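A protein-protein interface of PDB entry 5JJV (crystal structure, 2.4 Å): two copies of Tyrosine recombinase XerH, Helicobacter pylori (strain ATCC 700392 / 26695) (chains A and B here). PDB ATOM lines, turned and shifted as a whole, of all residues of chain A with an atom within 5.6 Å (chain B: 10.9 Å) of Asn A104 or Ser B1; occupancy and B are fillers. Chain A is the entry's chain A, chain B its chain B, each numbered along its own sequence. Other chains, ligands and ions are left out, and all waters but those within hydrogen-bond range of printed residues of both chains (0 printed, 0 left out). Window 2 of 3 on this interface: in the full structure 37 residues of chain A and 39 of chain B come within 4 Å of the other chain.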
ATOM      1  N   PHE A  99     -16.797   8.312  31.836  1.00  0.00           N
ATOM      2  CA  PHE A  99     -15.480   8.386  32.457  1.00  0.00           C
ATOM      3  C   PHE A  99     -15.562   8.103  33.953  1.00  0.00           C
ATOM      4  O   PHE A  99     -14.686   8.502  34.720  1.00  0.00           O
ATOM      5  CB  PHE A  99     -14.851   9.759  32.216  1.00  0.00           C
ATOM      6  N   ASN A 100     -16.620   7.407  34.358  1.00  0.00           N
ATOM      7  CA  ASN A 100     -16.852   7.107  35.765  1.00  0.00           C
ATOM      8  C   ASN A 100     -15.866   6.088  36.331  1.00  0.00           C
ATOM      9  O   ASN A 100     -15.550   6.117  37.521  1.00  0.00           O
ATOM     10  CB  ASN A 100     -18.283   6.599  35.964  1.00  0.00           C
ATOM     11  CG  ASN A 100     -18.566   6.201  37.401  1.00  0.00           C
ATOM     12  OD1 ASN A 100     -18.335   5.058  37.798  1.00  0.00           O
ATOM     13  ND2 ASN A 100     -19.072   7.144  38.187  1.00  0.00           N
ATOM     14  N   SER A 101     -15.379   5.191  35.479  1.00  0.00           N
ATOM     15  CA  SER A 101     -14.548   4.086  35.943  1.00  0.00           C
ATOM     16  C   SER A 101     -13.261   3.909  35.145  1.00  0.00           C
ATOM     17  O   SER A 101     -13.124   4.417  34.033  1.00  0.00           O
ATOM     18  CB  SER A 101     -15.347   2.781  35.907  1.00  0.00           C
ATOM     19  OG  SER A 101     -14.529   1.674  36.242  1.00  0.00           O
ATOM     20  N   LEU A 102     -12.324   3.172  35.732  1.00  0.00           N
ATOM     21  CA  LEU A 102     -11.076   2.829  35.068  1.00  0.00           C
ATOM     22  C   LEU A 102     -11.320   1.787  33.983  1.00  0.00           C
ATOM     23  O   LEU A 102     -10.491   1.595  33.093  1.00  0.00           O
ATOM     24  CB  LEU A 102     -10.056   2.307  36.081  1.00  0.00           C
ATOM     25  CG  LEU A 102      -9.618   3.269  37.187  1.00  0.00           C
ATOM     26  CD1 LEU A 102      -8.792   2.536  38.234  1.00  0.00           C
ATOM     27  CD2 LEU A 102      -8.833   4.431  36.601  1.00  0.00           C
ATOM     28  N   LYS A 103     -12.465   1.118  34.065  1.00  0.00           N
ATOM     29  CA  LYS A 103     -12.825   0.090  33.098  1.00  0.00           C
ATOM     30  C   LYS A 103     -13.161   0.690  31.738  1.00  0.00           C
ATOM     31  O   LYS A 103     -13.127  -0.004  30.722  1.00  0.00           O
ATOM     32  CB  LYS A 103     -14.006  -0.734  33.609  1.00  0.00           C
ATOM     33  CG  LYS A 103     -13.707  -1.537  34.860  1.00  0.00           C
ATOM     34  CD  LYS A 103     -14.946  -2.274  35.335  1.00  0.00           C
ATOM     35  CE  LYS A 103     -14.660  -3.102  36.575  1.00  0.00           C
ATOM     36  NZ  LYS A 103     -15.896  -3.752  37.091  1.00  0.00           N
ATOM     37  N   ASN A 104     -13.487   1.979  31.724  1.00  0.00           N
ATOM     38  CA  ASN A 104     -13.793   2.678  30.480  1.00  0.00           C
ATOM     39  C   ASN A 104     -12.567   2.812  29.580  1.00  0.00           C
ATOM     40  O   ASN A 104     -12.690   3.032  28.375  1.00  0.00           O
ATOM     41  CB  ASN A 104     -14.373   4.063  30.773  1.00  0.00           C
ATOM     42  CG  ASN A 104     -15.731   3.996  31.437  1.00  0.00           C
ATOM     43  OD1 ASN A 104     -15.932   4.542  32.522  1.00  0.00           O
ATOM     44  ND2 ASN A 104     -16.674   3.323  30.788  1.00  0.00           N
ATOM     45  N   ILE A 105     -11.387   2.681  30.175  1.00  0.00           N
ATOM     46  CA  ILE A 105     -10.144   2.806  29.429  1.00  0.00           C
ATOM     47  C   ILE A 105      -9.925   1.607  28.515  1.00  0.00           C
ATOM     48  O   ILE A 105      -9.668   0.497  28.978  1.00  0.00           O
ATOM     49  CB  ILE A 105      -8.931   2.946  30.365  1.00  0.00           C
ATOM     50  CG1 ILE A 105      -9.120   4.134  31.311  1.00  0.00           C
ATOM     51  CG2 ILE A 105      -7.653   3.106  29.555  1.00  0.00           C
ATOM     52  CD1 ILE A 105      -7.964   4.349  32.260  1.00  0.00           C
ATOM     53  N   ASP A 106     -10.043   1.840  27.212  1.00  0.00           N
ATOM     54  CA  ASP A 106      -9.721   0.827  26.216  1.00  0.00           C
ATOM     55  C   ASP A 106      -8.716   1.388  25.215  1.00  0.00           C
ATOM     56  O   ASP A 106      -8.248   2.516  25.369  1.00  0.00           O
ATOM     57  CB  ASP A 106     -10.985   0.337  25.502  1.00  0.00           C
ATOM     58  CG  ASP A 106     -11.862   1.473  25.007  1.00  0.00           C
ATOM     59  OD1 ASP A 106     -11.341   2.584  24.773  1.00  0.00           O
ATOM     60  OD2 ASP A 106     -13.081   1.250  24.844  1.00  0.00           O
ATOM     61  N   MET A 109      -9.750   4.737  23.535  1.00  0.00           N
ATOM     62  CA  MET A 109      -9.463   5.933  24.317  1.00  0.00           C
ATOM     63  C   MET A 109      -7.979   6.280  24.238  1.00  0.00           C
ATOM     64  O   MET A 109      -7.612   7.450  24.121  1.00  0.00           O
ATOM     65  CB  MET A 109      -9.880   5.745  25.776  1.00  0.00           C
ATOM     66  CG  MET A 109      -9.493   6.907  26.680  1.00  0.00           C
ATOM     67  SD  MET A 109      -9.777   6.581  28.429  1.00  0.00           S
ATOM     68  CE  MET A 109     -11.552   6.334  28.443  1.00  0.00           C
ATOM     69  N   TYR A 152      -9.605  -7.739  36.946  1.00  0.00           N
ATOM     70  CA  TYR A 152      -9.969  -7.132  35.672  1.00  0.00           C
ATOM     71  C   TYR A 152      -8.750  -7.096  34.759  1.00  0.00           C
ATOM     72  O   TYR A 152      -7.670  -6.675  35.173  1.00  0.00           O
ATOM     73  CB  TYR A 152     -10.527  -5.722  35.874  1.00  0.00           C
ATOM     74  CG  TYR A 152     -10.995  -5.063  34.595  1.00  0.00           C
ATOM     75  CD1 TYR A 152     -12.293  -5.243  34.134  1.00  0.00           C
ATOM     76  CD2 TYR A 152     -10.141  -4.261  33.848  1.00  0.00           C
ATOM     77  CE1 TYR A 152     -12.726  -4.644  32.965  1.00  0.00           C
ATOM     78  CE2 TYR A 152     -10.565  -3.660  32.678  1.00  0.00           C
ATOM     79  CZ  TYR A 152     -11.858  -3.854  32.241  1.00  0.00           C
ATOM     80  OH  TYR A 152     -12.288  -3.257  31.078  1.00  0.00           O
ATOM     81  N   SER B   1     -17.164   5.362  28.434  1.00  0.00           N
ATOM     82  CA  SER B   1     -16.652   6.539  27.743  1.00  0.00           C
ATOM     83  C   SER B   1     -16.635   6.319  26.234  1.00  0.00           C
ATOM     84  O   SER B   1     -17.395   6.945  25.496  1.00  0.00           O
ATOM     85  CB  SER B   1     -15.250   6.888  28.245  1.00  0.00           C
ATOM     86  OG  SER B   1     -14.734   8.027  27.576  1.00  0.00           O
ATOM     87  N   MET B   2     -15.761   5.427  25.779  1.00  0.00           N
ATOM     88  CA  MET B   2     -15.692   5.081  24.365  1.00  0.00           C
ATOM     89  C   MET B   2     -16.577   3.878  24.060  1.00  0.00           C
ATOM     90  O   MET B   2     -16.682   3.448  22.912  1.00  0.00           O
ATOM     91  CB  MET B   2     -14.250   4.796  23.944  1.00  0.00           C
ATOM     92  CG  MET B   2     -13.309   5.978  24.094  1.00  0.00           C
ATOM     93  SD  MET B   2     -13.909   7.478  23.292  1.00  0.00           S
ATOM     94  CE  MET B   2     -14.114   6.926  21.602  1.00  0.00           C
ATOM     95  N   LYS B   3     -17.209   3.337  25.098  1.00  0.00           N
ATOM     96  CA  LYS B   3     -18.122   2.212  24.931  1.00  0.00           C
ATOM     97  C   LYS B   3     -19.569   2.648  25.117  1.00  0.00           C
ATOM     98  O   LYS B   3     -19.892   3.393  26.041  1.00  0.00           O
ATOM     99  CB  LYS B   3     -17.785   1.088  25.913  1.00  0.00           C
ATOM    100  CG  LYS B   3     -16.436   0.431  25.672  1.00  0.00           C
ATOM    101  CD  LYS B   3     -16.293  -0.839  26.495  1.00  0.00           C
ATOM    102  CE  LYS B   3     -14.893  -1.419  26.383  1.00  0.00           C
ATOM    103  NZ  LYS B   3     -13.874  -0.514  26.980  1.00  0.00           N
ATOM    104  N   HIS B   4     -20.435   2.177  24.226  1.00  0.00           N
ATOM    105  CA  HIS B   4     -21.859   2.475  24.289  1.00  0.00           C
ATOM    106  C   HIS B   4     -22.654   1.218  23.964  1.00  0.00           C
ATOM    107  O   HIS B   4     -22.152   0.335  23.273  1.00  0.00           O
ATOM    108  CB  HIS B   4     -22.226   3.599  23.315  1.00  0.00           C
ATOM    109  CG  HIS B   4     -21.381   4.827  23.458  1.00  0.00           C
ATOM    110  ND1 HIS B   4     -20.165   4.970  22.827  1.00  0.00           N
ATOM    111  CD2 HIS B   4     -21.580   5.967  24.160  1.00  0.00           C
ATOM    112  CE1 HIS B   4     -19.649   6.148  23.133  1.00  0.00           C
ATOM    113  NE2 HIS B   4     -20.487   6.772  23.941  1.00  0.00           N
ATOM    114  N   PRO B   5     -23.895   1.126  24.467  1.00  0.00           N
ATOM    115  CA  PRO B   5     -24.756   0.004  24.075  1.00  0.00           C
ATOM    116  C   PRO B   5     -24.997  -0.013  22.568  1.00  0.00           C
ATOM    117  O   PRO B   5     -24.915   1.032  21.920  1.00  0.00           O
ATOM    118  CB  PRO B   5     -26.058   0.262  24.845  1.00  0.00           C
ATOM    119  CG  PRO B   5     -25.987   1.689  25.285  1.00  0.00           C
ATOM    120  CD  PRO B   5     -24.538   1.994  25.466  1.00  0.00           C
ATOM    121  N   GLU B   8     -28.911   2.534  20.924  1.00  0.00           N
ATOM    122  CA  GLU B   8     -29.260   3.646  21.801  1.00  0.00           C
ATOM    123  C   GLU B   8     -30.441   4.441  21.257  1.00  0.00           C
ATOM    124  O   GLU B   8     -31.106   5.166  21.996  1.00  0.00           O
ATOM    125  CB  GLU B   8     -28.060   4.573  21.992  1.00  0.00           C
ATOM    126  CG  GLU B   8     -26.903   3.947  22.744  1.00  0.00           C
ATOM    127  CD  GLU B   8     -25.726   4.889  22.893  1.00  0.00           C
ATOM    128  OE1 GLU B   8     -25.355   5.540  21.894  1.00  0.00           O
ATOM    129  OE2 GLU B   8     -25.172   4.982  24.009  1.00  0.00           O
ATOM    130  N   LEU B  18     -24.619   6.599  13.760  1.00  0.00           N
ATOM    131  CA  LEU B  18     -23.898   6.933  14.982  1.00  0.00           C
ATOM    132  C   LEU B  18     -22.605   6.131  15.114  1.00  0.00           C
ATOM    133  O   LEU B  18     -21.545   6.687  15.403  1.00  0.00           O
ATOM    134  CB  LEU B  18     -24.796   6.697  16.198  1.00  0.00           C
ATOM    135  CG  LEU B  18     -24.216   6.976  17.583  1.00  0.00           C
ATOM    136  CD1 LEU B  18     -23.720   8.409  17.683  1.00  0.00           C
ATOM    137  CD2 LEU B  18     -25.269   6.695  18.643  1.00  0.00           C
ATOM    138  N   TRP B  19     -22.700   4.821  14.898  1.00  0.00           N
ATOM    139  CA  TRP B  19     -21.541   3.942  15.000  1.00  0.00           C
ATOM    140  C   TRP B  19     -20.504   4.235  13.923  1.00  0.00           C
ATOM    141  O   TRP B  19     -19.301   4.147  14.173  1.00  0.00           O
ATOM    142  CB  TRP B  19     -21.969   2.476  14.919  1.00  0.00           C
ATOM    143  CG  TRP B  19     -22.506   1.936  16.207  1.00  0.00           C
ATOM    144  CD1 TRP B  19     -23.794   1.573  16.472  1.00  0.00           C
ATOM    145  CD2 TRP B  19     -21.766   1.706  17.410  1.00  0.00           C
ATOM    146  NE1 TRP B  19     -23.900   1.124  17.766  1.00  0.00           N
ATOM    147  CE2 TRP B  19     -22.670   1.196  18.364  1.00  0.00           C
ATOM    148  CE3 TRP B  19     -20.427   1.879  17.775  1.00  0.00           C
ATOM    149  CZ2 TRP B  19     -22.278   0.858  19.658  1.00  0.00           C
ATOM    150  CZ3 TRP B  19     -20.040   1.543  19.059  1.00  0.00           C
ATOM    151  CH2 TRP B  19     -20.962   1.039  19.986  1.00  0.00           C
ATOM    152  N   ARG B  22     -18.459   7.151  14.984  1.00  0.00           N
ATOM    153  CA  ARG B  22     -17.536   6.732  16.031  1.00  0.00           C
ATOM    154  C   ARG B  22     -16.326   6.007  15.451  1.00  0.00           C
ATOM    155  O   ARG B  22     -15.194   6.221  15.887  1.00  0.00           O
ATOM    156  CB  ARG B  22     -18.247   5.828  17.038  1.00  0.00           C
ATOM    157  CG  ARG B  22     -19.336   6.526  17.835  1.00  0.00           C
ATOM    158  CD  ARG B  22     -20.190   5.520  18.586  1.00  0.00           C
ATOM    159  NE  ARG B  22     -21.154   6.166  19.471  1.00  0.00           N
ATOM    160  CZ  ARG B  22     -22.118   5.523  20.119  1.00  0.00           C
ATOM    161  NH1 ARG B  22     -22.253   4.212  19.978  1.00  0.00           N
ATOM    162  NH2 ARG B  22     -22.951   6.190  20.907  1.00  0.00           N
ATOM    163  N   ARG B  25     -14.086   8.406  13.469  1.00  0.00           N
ATOM    164  CA  ARG B  25     -13.380   9.268  14.406  1.00  0.00           C
ATOM    165  C   ARG B  25     -12.176   8.539  14.986  1.00  0.00           C
ATOM    166  O   ARG B  25     -11.093   9.112  15.114  1.00  0.00           O
ATOM    167  CB  ARG B  25     -14.310   9.734  15.526  1.00  0.00           C
ATOM    168  CG  ARG B  25     -13.710  10.821  16.398  1.00  0.00           C
ATOM    169  CD  ARG B  25     -14.653  11.234  17.510  1.00  0.00           C
ATOM    170  NE  ARG B  25     -14.123  12.359  18.274  1.00  0.00           N
ATOM    171  CZ  ARG B  25     -13.253  12.243  19.272  1.00  0.00           C
ATOM    172  NH1 ARG B  25     -12.806  11.047  19.631  1.00  0.00           N
ATOM    173  NH2 ARG B  25     -12.826  13.325  19.910  1.00  0.00           N
ATOM    174  N   ASN B  50     -17.905  14.329  16.573  1.00  0.00           N
ATOM    175  CA  ASN B  50     -18.734  14.071  17.746  1.00  0.00           C
ATOM    176  C   ASN B  50     -20.096  14.745  17.636  1.00  0.00           C
ATOM    177  O   ASN B  50     -21.122  14.156  17.974  1.00  0.00           O
ATOM    178  CB  ASN B  50     -18.029  14.538  19.020  1.00  0.00           C
ATOM    179  CG  ASN B  50     -16.981  13.556  19.500  1.00  0.00           C
ATOM    180  OD1 ASN B  50     -17.138  12.342  19.361  1.00  0.00           O
ATOM    181  ND2 ASN B  50     -15.901  14.075  20.073  1.00  0.00           N
ATOM    182  N   TYR B 139     -15.143  -2.823  14.873  1.00  0.00           N
ATOM    183  CA  TYR B 139     -15.173  -1.757  15.868  1.00  0.00           C
ATOM    184  C   TYR B 139     -16.409  -1.882  16.754  1.00  0.00           C
ATOM    185  O   TYR B 139     -16.319  -1.794  17.979  1.00  0.00           O
ATOM    186  CB  TYR B 139     -15.148  -0.391  15.177  1.00  0.00           C
ATOM    187  CG  TYR B 139     -15.173   0.799  16.113  1.00  0.00           C
ATOM    188  CD1 TYR B 139     -16.376   1.370  16.512  1.00  0.00           C
ATOM    189  CD2 TYR B 139     -13.995   1.363  16.582  1.00  0.00           C
ATOM    190  CE1 TYR B 139     -16.404   2.459  17.362  1.00  0.00           C
ATOM    191  CE2 TYR B 139     -14.013   2.455  17.433  1.00  0.00           C
ATOM    192  CZ  TYR B 139     -15.220   2.998  17.818  1.00  0.00           C
ATOM    193  OH  TYR B 139     -15.245   4.083  18.664  1.00  0.00           O
ATOM    194  N   LYS B 142     -16.290  -4.653  19.240  1.00  0.00           N
ATOM    195  CA  LYS B 142     -15.375  -4.387  20.340  1.00  0.00           C
ATOM    196  C   LYS B 142     -15.884  -3.289  21.270  1.00  0.00           C
ATOM    197  O   LYS B 142     -15.536  -3.260  22.450  1.00  0.00           O
ATOM    198  CB  LYS B 142     -13.994  -4.009  19.797  1.00  0.00           C
ATOM    199  N   GLN B 143     -16.716  -2.394  20.746  1.00  0.00           N
ATOM    200  CA  GLN B 143     -17.099  -1.199  21.493  1.00  0.00           C
ATOM    201  C   GLN B 143     -18.543  -1.191  22.001  1.00  0.00           C
ATOM    202  O   GLN B 143     -18.919  -0.302  22.765  1.00  0.00           O
ATOM    203  CB  GLN B 143     -16.863   0.046  20.633  1.00  0.00           C
ATOM    204  CG  GLN B 143     -15.409   0.252  20.241  1.00  0.00           C
ATOM    205  CD  GLN B 143     -14.481   0.244  21.437  1.00  0.00           C
ATOM    206  OE1 GLN B 143     -13.636  -0.641  21.575  1.00  0.00           O
ATOM    207  NE2 GLN B 143     -14.626   1.235  22.309  1.00  0.00           N
ATOM    208  N   ASN B 144     -19.352  -2.161  21.589  1.00  0.00           N
ATOM    209  CA  ASN B 144     -20.739  -2.197  22.046  1.00  0.00           C
ATOM    210  C   ASN B 144     -20.847  -2.888  23.404  1.00  0.00           C
ATOM    211  O   ASN B 144     -20.216  -3.919  23.639  1.00  0.00           O
ATOM    212  CB  ASN B 144     -21.645  -2.877  21.009  1.00  0.00           C
ATOM    213  CG  ASN B 144     -21.721  -4.382  21.184  1.00  0.00           C
ATOM    214  OD1 ASN B 144     -22.641  -4.899  21.820  1.00  0.00           O
ATOM    215  ND2 ASN B 144     -20.756  -5.094  20.616  1.00  0.00           N
ATOM    216  N   GLN B 145     -21.636  -2.301  24.300  1.00  0.00           N
ATOM    217  CA  GLN B 145     -21.755  -2.795  25.670  1.00  0.00           C
ATOM    218  C   GLN B 145     -22.906  -2.109  26.405  1.00  0.00           C
ATOM    219  O   GLN B 145     -22.897  -0.889  26.580  1.00  0.00           O
ATOM    220  CB  GLN B 145     -20.443  -2.572  26.427  1.00  0.00           C
ATOM    221  CG  GLN B 145     -20.304  -3.387  27.698  1.00  0.00           C
ATOM    222  CD  GLN B 145     -18.986  -3.135  28.404  1.00  0.00           C
ATOM    223  OE1 GLN B 145     -18.595  -1.988  28.621  1.00  0.00           O
ATOM    224  NE2 GLN B 145     -18.290  -4.208  28.759  1.00  0.00           N
ATOM    225  N   ASP B 146     -23.890  -2.891  26.843  1.00  0.00           N
ATOM    226  CA  ASP B 146     -25.066  -2.333  27.508  1.00  0.00           C
ATOM    227  C   ASP B 146     -24.805  -2.006  28.977  1.00  0.00           C
ATOM    228  O   ASP B 146     -23.661  -2.011  29.434  1.00  0.00           O
ATOM    229  CB  ASP B 146     -26.260  -3.289  27.392  1.00  0.00           C
ATOM    230  CG  ASP B 146     -25.980  -4.666  27.977  1.00  0.00           C
ATOM    231  OD1 ASP B 146     -24.967  -4.837  28.685  1.00  0.00           O
ATOM    232  OD2 ASP B 146     -26.791  -5.584  27.732  1.00  0.00           O
ATOM    233  N   GLU B 147     -25.879  -1.735  29.712  1.00  0.00           N
ATOM    234  CA  GLU B 147     -25.782  -1.407  31.130  1.00  0.00           C
ATOM    235  C   GLU B 147     -25.368  -2.620  31.956  1.00  0.00           C
ATOM    236  O   GLU B 147     -24.806  -2.479  33.044  1.00  0.00           O
ATOM    237  CB  GLU B 147     -27.113  -0.853  31.641  1.00  0.00           C
ATOM    238  N   GLU B 149     -23.172  -4.783  31.014  1.00  0.00           N
ATOM    239  CA  GLU B 149     -21.860  -5.165  30.489  1.00  0.00           C
ATOM    240  C   GLU B 149     -21.944  -6.311  29.481  1.00  0.00           C
ATOM    241  O   GLU B 149     -20.971  -7.037  29.273  1.00  0.00           O
ATOM    242  CB  GLU B 149     -20.913  -5.543  31.632  1.00  0.00           C
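The side-chain hydroxyl of Ser A101 lies within hydrogen-bond range of the backbone NH of Lys A103 (3.1 Å). N of Ser A101 sits at hydrogen-bond distance from OD1 of Asn A104 (3.1 Å). The backbone carbonyl oxygen (O) of Lys A103 sits at hydrogen-bond distance from the side-chain hydroxyl (OH) of Tyr A152, at 3.4 Å. The backbone NH (N) of Met A109 is in hydrogen-bond range of the side-chain carboxylate (OD1) of Asp A106, 2.9 Å away. The backbone carbonyl oxygen of Ser B1 lies close to a ring nitrogen (NE2) of His B4 (3.5 Å). The backbone NH of His B4 lies within hydrogen-bond range of the backbone carbonyl oxygen of Gln B143, at 3.3 Å.
The side-chain amide nitrogen (ND2) of Asn A104 lies close to the backbone NH (N) of Ser B1 (3.2 Å). NZ of Lys B3 lies within salt-bridge range of OD2 of Asp A106. The side-chain amide nitrogen (NE2) of Gln B143 sits at hydrogen-bond distance from the side-chain carboxylate (OD2) of Asp A106, at 3.0 Å.
Printed residues of chain B within 4 Å of Asn A104: Ser B1 and Lys B3. Of chain A, only Asn A104 (3.2 Å) and Met A109 (3.7 Å) come within 4 Å of Ser B1. No residue of chain B comes within 4 Å of Ile A105. Asp A106 touches just these residues of chain B: Met B2, Lys B3 and Gln B143. Printed residues of chain A within 4 Å of Lys B3: Lys A103 (3.8 Å), Asn A104 (3.99 Å) and Asp A106 (2.9 Å). Of the printed residues of chain B, Lys A103 touches Lys B3. Printed residues of chain A within 4 Å of Gln B143: Asp A106 (3.0 Å). Printed residues of chain B within 4 Å of Met A109: Ser B1 and Met B2. Of the printed residues of chain A, Met B2 touches Asp A106 and Met A109. Leu A102 touches none of the printed residues of chain B. The nearest residue of chain A that does not touch Ser B1 is Phe A99 (4.2 Å).
No position is printed for both chains. Of the 8 pairs that touch across the chains among the printed residues, none has its exchanged pair printed and touching as well.
Among the printed residues, pairs that only touch across the chains: Met A109 with Ser B1 (3.7 Å), Asp A106 with Met B2 (3.7 Å), Met A109 with Met B2 (3.8 Å), Lys A103 with Lys B3 (3.8 Å) and Asn A104 with Lys B3 (3.99 Å).
Of the 19 printed residues of chain B, 4 touch a printed residue of chain A. Hydrophobic or aromatic side chains of chain B that line the printed part of chain A: Met B2. Of the 10 printed residues of chain A, 4 touch a printed residue of chain B. Among the printed residues, Asp or Glu carboxylates within 4 Å of a Lys or Arg side-chain nitrogen of the other chain: Asp A106 with Lys B3 (2.9 Å).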
